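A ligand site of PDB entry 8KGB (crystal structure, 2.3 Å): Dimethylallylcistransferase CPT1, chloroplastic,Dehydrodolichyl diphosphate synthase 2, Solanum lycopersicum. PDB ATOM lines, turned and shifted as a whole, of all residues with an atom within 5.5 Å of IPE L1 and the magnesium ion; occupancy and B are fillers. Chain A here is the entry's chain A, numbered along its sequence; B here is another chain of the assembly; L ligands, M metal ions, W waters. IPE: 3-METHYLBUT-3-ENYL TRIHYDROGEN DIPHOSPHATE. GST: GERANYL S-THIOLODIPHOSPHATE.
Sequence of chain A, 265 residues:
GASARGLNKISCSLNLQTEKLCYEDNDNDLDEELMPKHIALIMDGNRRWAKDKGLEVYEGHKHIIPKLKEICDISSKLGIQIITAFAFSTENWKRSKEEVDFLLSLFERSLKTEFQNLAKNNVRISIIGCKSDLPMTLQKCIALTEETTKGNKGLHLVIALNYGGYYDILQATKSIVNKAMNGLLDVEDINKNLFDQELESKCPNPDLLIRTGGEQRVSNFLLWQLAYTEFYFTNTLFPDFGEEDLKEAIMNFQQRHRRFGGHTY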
ATOM      1  N   ILE A  42       7.690  15.340 -15.563  1.00  0.00           N
ATOM      2  CA  ILE A  42       8.849  15.294 -14.640  1.00  0.00           C
ATOM      3  C   ILE A  42       8.496  14.313 -13.521  1.00  0.00           C
ATOM      4  O   ILE A  42       7.601  14.633 -12.741  1.00  0.00           O
ATOM      5  CB  ILE A  42       9.189  16.701 -14.123  1.00  0.00           C
ATOM      6  CG1 ILE A  42       9.564  17.635 -15.269  1.00  0.00           C
ATOM      7  CG2 ILE A  42      10.288  16.622 -13.079  1.00  0.00           C
ATOM      8  CD1 ILE A  42       9.856  19.053 -14.840  1.00  0.00           C
ATOM      9  N   MET A  43       9.188  13.177 -13.457  1.00  0.00           N
ATOM     10  CA  MET A  43       8.774  12.013 -12.616  1.00  0.00           C
ATOM     11  C   MET A  43       9.473  12.114 -11.260  1.00  0.00           C
ATOM     12  O   MET A  43      10.449  11.372 -11.008  1.00  0.00           O
ATOM     13  CB  MET A  43       9.076  10.697 -13.334  1.00  0.00           C
ATOM     14  CG  MET A  43       8.375  10.631 -14.705  1.00  0.00           C
ATOM     15  SD  MET A  43       8.582   9.120 -15.680  1.00  0.00           S
ATOM     16  CE  MET A  43      10.374   9.078 -15.882  1.00  0.00           C
ATOM     17  N   ASP A  44       8.984  13.035 -10.424  1.00  0.00           N
ATOM     18  CA  ASP A  44       9.720  13.483  -9.218  1.00  0.00           C
ATOM     19  C   ASP A  44       9.000  12.996  -7.967  1.00  0.00           C
ATOM     20  O   ASP A  44       7.775  12.891  -7.986  1.00  0.00           O
ATOM     21  CB  ASP A  44       9.871  15.008  -9.199  1.00  0.00           C
ATOM     22  CG  ASP A  44      10.880  15.481  -8.177  1.00  0.00           C
ATOM     23  OD1 ASP A  44      11.783  14.698  -7.859  1.00  0.00           O
ATOM     24  OD2 ASP A  44      10.757  16.644  -7.697  1.00  0.00           O
ATOM     25  N   GLY A  45       9.762  12.747  -6.906  1.00  0.00           N
ATOM     26  CA  GLY A  45       9.231  12.445  -5.565  1.00  0.00           C
ATOM     27  C   GLY A  45       9.317  10.976  -5.188  1.00  0.00           C
ATOM     28  O   GLY A  45       8.649  10.588  -4.223  1.00  0.00           O
ATOM     29  N   ARG A  48      10.902  10.253  -1.520  1.00  0.00           N
ATOM     30  CA  ARG A  48      10.049  10.671  -0.396  1.00  0.00           C
ATOM     31  C   ARG A  48       8.827   9.748  -0.325  1.00  0.00           C
ATOM     32  O   ARG A  48       8.270   9.580   0.781  1.00  0.00           O
ATOM     33  CB  ARG A  48       9.596  12.131  -0.545  1.00  0.00           C
ATOM     34  CG  ARG A  48      10.698  13.153  -0.333  1.00  0.00           C
ATOM     35  CD  ARG A  48      10.247  14.512  -0.870  1.00  0.00           C
ATOM     36  NE  ARG A  48      10.435  14.639  -2.314  1.00  0.00           N
ATOM     37  CZ  ARG A  48       9.828  15.520  -3.112  1.00  0.00           C
ATOM     38  NH1 ARG A  48       8.946  16.372  -2.617  1.00  0.00           N
ATOM     39  NH2 ARG A  48      10.088  15.540  -4.409  1.00  0.00           N
ATOM     40  N   PHE A  86      10.975  12.694 -17.977  1.00  0.00           N
ATOM     41  CA  PHE A  86      12.302  13.048 -17.431  1.00  0.00           C
ATOM     42  C   PHE A  86      12.711  11.913 -16.496  1.00  0.00           C
ATOM     43  O   PHE A  86      12.105  11.794 -15.419  1.00  0.00           O
ATOM     44  CB  PHE A  86      12.269  14.406 -16.740  1.00  0.00           C
ATOM     45  CG  PHE A  86      13.574  15.180 -16.707  1.00  0.00           C
ATOM     46  CD1 PHE A  86      14.701  14.745 -17.392  1.00  0.00           C
ATOM     47  CD2 PHE A  86      13.671  16.362 -15.990  1.00  0.00           C
ATOM     48  CE1 PHE A  86      15.886  15.454 -17.367  1.00  0.00           C
ATOM     49  CE2 PHE A  86      14.852  17.093 -15.969  1.00  0.00           C
ATOM     50  CZ  PHE A  86      15.969  16.638 -16.652  1.00  0.00           C
ATOM     51  N   ALA A  87      13.688  11.097 -16.898  1.00  0.00           N
ATOM     52  CA  ALA A  87      14.107   9.915 -16.133  1.00  0.00           C
ATOM     53  C   ALA A  87      15.450  10.131 -15.421  1.00  0.00           C
ATOM     54  O   ALA A  87      15.625   9.551 -14.345  1.00  0.00           O
ATOM     55  CB  ALA A  87      14.175   8.710 -17.021  1.00  0.00           C
ATOM     56  N   PHE A  88      16.369  10.896 -16.017  1.00  0.00           N
ATOM     57  CA  PHE A  88      17.705  11.127 -15.422  1.00  0.00           C
ATOM     58  C   PHE A  88      18.287  12.402 -16.016  1.00  0.00           C
ATOM     59  O   PHE A  88      18.500  12.439 -17.238  1.00  0.00           O
ATOM     60  CB  PHE A  88      18.595   9.913 -15.666  1.00  0.00           C
ATOM     61  CG  PHE A  88      20.015  10.015 -15.161  1.00  0.00           C
ATOM     62  CD1 PHE A  88      20.277  10.255 -13.825  1.00  0.00           C
ATOM     63  CD2 PHE A  88      21.088   9.835 -16.017  1.00  0.00           C
ATOM     64  CE1 PHE A  88      21.581  10.343 -13.368  1.00  0.00           C
ATOM     65  CE2 PHE A  88      22.397   9.910 -15.553  1.00  0.00           C
ATOM     66  CZ  PHE A  88      22.635  10.186 -14.230  1.00  0.00           C
ATOM     67  N   SER A  89      18.533  13.406 -15.174  1.00  0.00           N
ATOM     68  CA  SER A  89      19.035  14.723 -15.614  1.00  0.00           C
ATOM     69  C   SER A  89      20.562  14.761 -15.549  1.00  0.00           C
ATOM     70  O   SER A  89      21.179  13.933 -14.856  1.00  0.00           O
ATOM     71  CB  SER A  89      18.489  15.847 -14.799  1.00  0.00           C
ATOM     72  OG  SER A  89      19.368  16.156 -13.740  1.00  0.00           O
ATOM     73  N   ASN A  92      21.939  15.044 -11.980  1.00  0.00           N
ATOM     74  CA  ASN A  92      21.785  13.890 -11.056  1.00  0.00           C
ATOM     75  C   ASN A  92      23.136  13.174 -10.873  1.00  0.00           C
ATOM     76  O   ASN A  92      23.306  12.478  -9.872  1.00  0.00           O
ATOM     77  CB  ASN A  92      20.669  12.942 -11.514  1.00  0.00           C
ATOM     78  CG  ASN A  92      19.259  13.480 -11.378  1.00  0.00           C
ATOM     79  OD1 ASN A  92      18.402  13.178 -12.189  1.00  0.00           O
ATOM     80  ND2 ASN A  92      18.972  14.254 -10.335  1.00  0.00           N
ATOM     81  N   ARG A  95      24.769  13.131  -7.327  1.00  0.00           N
ATOM     82  CA  ARG A  95      24.386  12.185  -6.266  1.00  0.00           C
ATOM     83  C   ARG A  95      25.511  11.169  -6.063  1.00  0.00           C
ATOM     84  O   ARG A  95      26.521  11.207  -6.821  1.00  0.00           O
ATOM     85  CB  ARG A  95      23.045  11.531  -6.605  1.00  0.00           C
ATOM     86  CG  ARG A  95      21.911  12.530  -6.732  1.00  0.00           C
ATOM     87  CD  ARG A  95      20.604  11.931  -7.191  1.00  0.00           C
ATOM     88  NE  ARG A  95      19.555  12.943  -7.300  1.00  0.00           N
ATOM     89  CZ  ARG A  95      18.242  12.702  -7.378  1.00  0.00           C
ATOM     90  NH1 ARG A  95      17.789  11.466  -7.375  1.00  0.00           N
ATOM     91  NH2 ARG A  95      17.393  13.711  -7.477  1.00  0.00           N
ATOM     92  N   ARG A 211       4.409  18.080 -13.490  1.00  0.00           N
ATOM     93  CA  ARG A 211       5.487  17.747 -12.546  1.00  0.00           C
ATOM     94  C   ARG A 211       4.840  17.258 -11.259  1.00  0.00           C
ATOM     95  O   ARG A 211       4.107  18.041 -10.624  1.00  0.00           O
ATOM     96  CB  ARG A 211       6.412  18.938 -12.267  1.00  0.00           C
ATOM     97  CG  ARG A 211       7.473  18.605 -11.223  1.00  0.00           C
ATOM     98  CD  ARG A 211       8.578  19.626 -11.150  1.00  0.00           C
ATOM     99  NE  ARG A 211       9.613  19.204 -10.211  1.00  0.00           N
ATOM    100  CZ  ARG A 211      10.913  19.385 -10.375  1.00  0.00           C
ATOM    101  NH1 ARG A 211      11.377  20.048 -11.427  1.00  0.00           N
ATOM    102  NH2 ARG A 211      11.758  18.940  -9.470  1.00  0.00           N
ATOM    103  N   GLU A 215       7.331  20.286  -6.254  1.00  0.00           N
ATOM    104  CA  GLU A 215       8.272  21.417  -6.462  1.00  0.00           C
ATOM    105  C   GLU A 215       7.763  22.269  -7.622  1.00  0.00           C
ATOM    106  O   GLU A 215       7.239  21.712  -8.618  1.00  0.00           O
ATOM    107  CB  GLU A 215       9.688  20.928  -6.726  1.00  0.00           C
ATOM    108  CG  GLU A 215      10.154  19.882  -5.747  1.00  0.00           C
ATOM    109  CD  GLU A 215      10.152  20.306  -4.293  1.00  0.00           C
ATOM    110  OE1 GLU A 215      10.275  21.524  -4.034  1.00  0.00           O
ATOM    111  OE2 GLU A 215      10.060  19.416  -3.421  1.00  0.00           O
ATOM    112  N   ARG A 217       9.140  24.234 -10.190  1.00  0.00           N
ATOM    113  CA  ARG A 217      10.393  24.502 -10.933  1.00  0.00           C
ATOM    114  C   ARG A 217      10.540  23.449 -12.025  1.00  0.00           C
ATOM    115  O   ARG A 217       9.855  22.395 -12.000  1.00  0.00           O
ATOM    116  CB  ARG A 217      11.618  24.464 -10.017  1.00  0.00           C
ATOM    117  CG  ARG A 217      11.706  23.219  -9.161  1.00  0.00           C
ATOM    118  CD  ARG A 217      13.011  23.263  -8.404  1.00  0.00           C
ATOM    119  NE  ARG A 217      13.269  22.144  -7.509  1.00  0.00           N
ATOM    120  CZ  ARG A 217      13.203  22.180  -6.185  1.00  0.00           C
ATOM    121  NH1 ARG A 217      12.752  23.267  -5.557  1.00  0.00           N
ATOM    122  NH2 ARG A 217      13.558  21.118  -5.481  1.00  0.00           N
ATOM    123  N   SER A 219      13.867  22.412 -13.313  1.00  0.00           N
ATOM    124  CA  SER A 219      15.085  21.582 -13.091  1.00  0.00           C
ATOM    125  C   SER A 219      15.763  21.226 -14.413  1.00  0.00           C
ATOM    126  O   SER A 219      16.129  20.059 -14.602  1.00  0.00           O
ATOM    127  CB  SER A 219      14.768  20.325 -12.315  1.00  0.00           C
ATOM    128  OG  SER A 219      14.071  20.617 -11.120  1.00  0.00           O
ATOM    129  N   TYR B 228      16.876  26.525 -12.989  1.00  0.00           N
ATOM    130  CA  TYR B 228      16.671  26.068 -11.580  1.00  0.00           C
ATOM    131  C   TYR B 228      15.973  27.144 -10.746  1.00  0.00           C
ATOM    132  O   TYR B 228      15.969  27.042  -9.511  1.00  0.00           O
ATOM    133  CB  TYR B 228      17.997  25.579 -10.972  1.00  0.00           C
ATOM    134  CG  TYR B 228      18.333  24.153 -11.331  1.00  0.00           C
ATOM    135  CD1 TYR B 228      17.685  23.108 -10.695  1.00  0.00           C
ATOM    136  CD2 TYR B 228      19.232  23.830 -12.338  1.00  0.00           C
ATOM    137  CE1 TYR B 228      17.941  21.784 -11.034  1.00  0.00           C
ATOM    138  CE2 TYR B 228      19.485  22.512 -12.699  1.00  0.00           C
ATOM    139  CZ  TYR B 228      18.841  21.481 -12.037  1.00  0.00           C
ATOM    140  OH  TYR B 228      19.061  20.160 -12.376  1.00  0.00           O
ATOM    141  N   ARG B 259      17.476  21.776  -4.423  1.00  0.00           N
ATOM    142  CA  ARG B 259      18.435  20.643  -4.395  1.00  0.00           C
ATOM    143  C   ARG B 259      19.366  20.671  -5.611  1.00  0.00           C
ATOM    144  O   ARG B 259      20.468  20.104  -5.489  1.00  0.00           O
ATOM    145  CB  ARG B 259      17.671  19.323  -4.308  1.00  0.00           C
ATOM    146  CG  ARG B 259      16.871  19.121  -3.029  1.00  0.00           C
ATOM    147  CD  ARG B 259      15.964  17.895  -3.106  1.00  0.00           C
ATOM    148  NE  ARG B 259      14.704  18.222  -2.455  1.00  0.00           N
ATOM    149  CZ  ARG B 259      13.493  18.099  -3.011  1.00  0.00           C
ATOM    150  NH1 ARG B 259      13.336  17.554  -4.197  1.00  0.00           N
ATOM    151  NH2 ARG B 259      12.428  18.491  -2.331  1.00  0.00           N
ATOM    152  N   PHE B 260      18.963  21.290  -6.717  1.00  0.00           N
ATOM    153  CA  PHE B 260      19.817  21.433  -7.924  1.00  0.00           C
ATOM    154  C   PHE B 260      20.234  20.054  -8.426  1.00  0.00           C
ATOM    155  O   PHE B 260      21.372  19.911  -8.946  1.00  0.00           O
ATOM    156  CB  PHE B 260      21.050  22.273  -7.613  1.00  0.00           C
ATOM    157  CG  PHE B 260      20.711  23.638  -7.068  1.00  0.00           C
ATOM    158  CD1 PHE B 260      20.160  24.605  -7.896  1.00  0.00           C
ATOM    159  CD2 PHE B 260      20.903  23.932  -5.721  1.00  0.00           C
ATOM    160  CE1 PHE B 260      19.834  25.857  -7.402  1.00  0.00           C
ATOM    161  CE2 PHE B 260      20.555  25.185  -5.223  1.00  0.00           C
ATOM    162  CZ  PHE B 260      20.026  26.141  -6.056  1.00  0.00           C
ATOM    163  N   GLY B 261      19.340  19.068  -8.289  1.00  0.00           N
ATOM    164  CA  GLY B 261      19.589  17.712  -8.806  1.00  0.00           C
ATOM    165  C   GLY B 261      20.335  16.824  -7.820  1.00  0.00           C
ATOM    166  O   GLY B 261      20.461  15.616  -8.139  1.00  0.00           O
ATOM    167  N   GLY B 262      20.771  17.352  -6.671  1.00  0.00           N
ATOM    168  CA  GLY B 262      21.548  16.574  -5.679  1.00  0.00           C
ATOM    169  C   GLY B 262      20.694  16.030  -4.561  1.00  0.00           C
ATOM    170  O   GLY B 262      19.468  16.268  -4.554  1.00  0.00           O
ATOM    171  N   HIS B 263      21.322  15.296  -3.641  1.00  0.00           N
ATOM    172  CA  HIS B 263      20.642  14.599  -2.520  1.00  0.00           C
ATOM    173  C   HIS B 263      21.421  14.768  -1.216  1.00  0.00           C
ATOM    174  O   HIS B 263      22.674  14.895  -1.260  1.00  0.00           O
ATOM    175  CB  HIS B 263      20.462  13.104  -2.811  1.00  0.00           C
ATOM    176  CG  HIS B 263      19.086  12.740  -3.251  1.00  0.00           C
ATOM    177  ND1 HIS B 263      18.818  11.535  -3.867  1.00  0.00           N
ATOM    178  CD2 HIS B 263      17.899  13.399  -3.164  1.00  0.00           C
ATOM    179  CE1 HIS B 263      17.526  11.459  -4.143  1.00  0.00           C
ATOM    180  NE2 HIS B 263      16.937  12.590  -3.732  1.00  0.00           N
HETATM  181  C1  IPE L   1      13.696  15.466 -11.178  1.00  0.00           C
HETATM  182  O1  IPE L   1      14.088  16.650 -10.542  1.00  0.00           O
HETATM  183  C2  IPE L   1      14.661  15.123 -12.250  1.00  0.00           C
HETATM  184  C3  IPE L   1      14.171  13.883 -12.932  1.00  0.00           C
HETATM  185  C4  IPE L   1      12.901  13.493 -12.805  1.00  0.00           C
HETATM  186  C5  IPE L   1      15.184  13.090 -13.690  1.00  0.00           C
HETATM  187  PA  IPE L   1      15.209  16.601  -9.407  1.00  0.00           P
HETATM  188  O1A IPE L   1      16.555  16.281  -9.966  1.00  0.00           O
HETATM  189  O2A IPE L   1      14.673  15.881  -8.219  1.00  0.00           O
HETATM  190  O3A IPE L   1      15.194  18.185  -9.195  1.00  0.00           O
HETATM  191  PB  IPE L   1      15.495  19.219  -8.034  1.00  0.00           P
HETATM  192  O1B IPE L   1      14.380  18.954  -7.050  1.00  0.00           O
HETATM  193  O2B IPE L   1      15.425  20.573  -8.689  1.00  0.00           O
HETATM  194  O3B IPE L   1      16.890  18.883  -7.536  1.00  0.00           O
HETATM  195  PA  GST L   2      12.831  12.931  -4.393  1.00  0.00           P
HETATM  196  O1A GST L   2      11.712  12.394  -3.524  1.00  0.00           O
HETATM  197  O2A GST L   2      12.414  14.113  -5.209  1.00  0.00           O
HETATM  198  O3A GST L   2      14.138  13.148  -3.680  1.00  0.00           O
HETATM  199  O1B GST L   2      13.075  11.743  -5.449  1.00  0.00           O
HETATM  200  PB  GST L   2      14.039  11.718  -6.713  1.00  0.00           P
HETATM  201  O2B GST L   2      14.575  13.101  -6.986  1.00  0.00           O
HETATM  202  O3B GST L   2      15.088  10.672  -6.539  1.00  0.00           O
HETATM  203  S1  GST L   2      12.640  11.194  -8.161  1.00  0.00           S
HETATM  204  C1  GST L   2      13.189  12.213  -9.556  1.00  0.00           C
HETATM  205  C2  GST L   2      14.554  11.847 -10.003  1.00  0.00           C
HETATM  206  C3  GST L   2      14.849  10.749 -10.686  1.00  0.00           C
HETATM  207  C10 GST L   2      13.824   9.724 -11.090  1.00  0.00           C
HETATM  208  C4  GST L   2      16.250  10.438 -11.107  1.00  0.00           C
HETATM  209  C5  GST L   2      16.680   9.039 -10.715  1.00  0.00           C
HETATM  210  C6  GST L   2      18.168   8.865 -10.702  1.00  0.00           C
HETATM  211  C7  GST L   2      18.916   8.104 -11.490  1.00  0.00           C
HETATM  212  C9  GST L   2      20.392   7.928 -11.282  1.00  0.00           C
HETATM  213  C8  GST L   2      18.349   7.353 -12.667  1.00  0.00           C
HETATM  214 MG    MG M   1      13.512  14.877  -6.741  1.00  0.00          MG
HETATM  215  O   HOH W   1      17.452  16.422  -6.284  1.00  0.00           O
HETATM  216  O   HOH W   2      16.246  22.549  -7.130  1.00  0.00           O
HETATM  217  O   HOH W   3      12.888  16.999  -6.354  1.00  0.00           O
HETATM  218  O   HOH W   4      18.006  17.793 -11.877  1.00  0.00           O
HETATM  219  O   HOH W   5      15.097  15.415  -5.357  1.00  0.00           O
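NE2 of His 263 of chain B lies within hydrogen-bond range of O3A of GST L2.
The backbone NH (N) of Gly 261 of chain B sits at hydrogen-bond distance from an oxygen (O3B) of IPE L1.
The guanidinium group (NH1) of Arg 259 of chain B lies within salt-bridge range of an oxygen (O1B) of IPE L1, 3.3 Å away.
The backbone NH (N) of Phe 260 of chain B sits at hydrogen-bond distance from an oxygen (O3B) of IPE L1, 3.3 Å away.
NH1 of Arg 259 of chain B lies close to O2A of GST L2 (3.7 Å).
NH2 of Arg 95 lies within salt-bridge range of O1A of IPE L1 (3.7 Å).
N of Arg 48 sits at hydrogen-bond distance from O1A of GST L2 (3.0 Å).
S1 of GST L2 sits close to N of Gly 45 (3.5 Å).
NH1 of Arg 95 is in salt-bridge range of O3B of GST L2 (2.9 Å).
The side-chain amide nitrogen of Asn 92 lies within hydrogen-bond range of an oxygen (O1A) of IPE L1 (3.2 Å).
An oxygen (O1B) of IPE L1 is in salt-bridge range of the guanidinium group (NH2) of Arg 217.
OG of Ser 219 is in hydrogen-bond range of O2B of IPE L1 (2.8 Å).
O1B of IPE L1 is in salt-bridge range of NH2 of Arg 211, at 3.6 Å.
NE of Arg 48 is in salt-bridge range of O1A of GST L2, 2.9 Å away.
The side-chain carboxylate (OE1) of Glu 215 is in salt-bridge range of the guanidinium group (NH1) of Arg 217.
ND2 of Asn 92 sits at hydrogen-bond distance from O of Gly 261 of chain B, 3.0 Å away.
OD2 of Asp 44 lies within salt-bridge range of NH2 of Arg 48, 3.5 Å away.
The guanidinium group of Arg 259 of chain B is in salt-bridge range of the side-chain carboxylate of Glu 215, at 2.8 Å.
The side-chain carboxylate (OD2) of Asp 44 lies within salt-bridge range of the guanidinium group (NH2) of Arg 211, 3.1 Å away.
ND2 of Asn 92 sits close to NH2 of Arg 95 (3.3 Å).
O of Arg 217 is in hydrogen-bond range of NH1 of Arg 211.
The side-chain amide oxygen (OD1) of Asn 92 lies within hydrogen-bond range of the backbone NH (N) of Ser 89.
Residues that only touch IPE L1: Phe 86 (3.2 Å), Phe 88 (3.4 Å), Ala 87 (3.4 Å), Tyr 228 of chain B (3.6 Å), Ser 89 (3.7 Å) and Met 43 (3.7 Å).
Hydrophobic or aromatic side chains within 4 Å of IPE L1: Phe 86 and Tyr 228 of chain B.
15 residues have an atom within 4 Å of IPE L1: Met 43, Asp 44, Phe 86, Ala 87, Phe 88, Ser 89, Asn 92, Arg 95, Arg 211, Arg 217, Ser 219, Tyr 228 of chain B, Arg 259 of chain B, Phe 260 of chain B and Gly 261 of chain B.
The nearest printed residue that does not touch IPE L1 is Ile 42 (4.1 Å).
Residues that only touch the magnesium ion: Arg 259 of chain B.
Two residues have an atom within 4 Å of the magnesium ion: Asp 44 and Arg 259 of chain B.
The nearest printed residue that does not touch the magnesium ion is Arg 95 (4.1 Å).
The magnesium ion is bound by an oxygen (O2A) of GST L2, 2.0 Å away.
The magnesium ion is bound by the side-chain carboxylate (OD1) of Asp 44, at 2.1 Å.
An oxygen (O2B) of GST L2 is bound to the magnesium ion (2.1 Å).
The magnesium ion is bound by O2A of IPE L1.
Water W5 binds the magnesium ion (2.2 Å).
The magnesium ion is bound by water W3.
The magnesium ion has six donor atoms within binding distance.
Water W5 lies within hydrogen-bond range of an oxygen (O3A) of GST L2 (3.0 Å) and the guanidinium group (NH1) of Arg 259 of chain B (3.0 Å).
Water W3 lies within hydrogen-bond range of the side-chain carboxylate (OD2) of Asp 44 (2.5 Å) and an oxygen (O1B) of IPE L1 (2.6 Å).
Water W1 lies within hydrogen-bond range of O of Gly 262 of chain B (2.7 Å), O3B of IPE L1 (2.8 Å) and NH2 of Arg 95 (3.0 Å).
Water W4 lies within hydrogen-bond range of the side-chain hydroxyl (OH) of Tyr 228 of chain B (2.6 Å), the side-chain hydroxyl (OG) of Ser 89 (2.8 Å) and an oxygen (O1A) of IPE L1 (2.8 Å).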
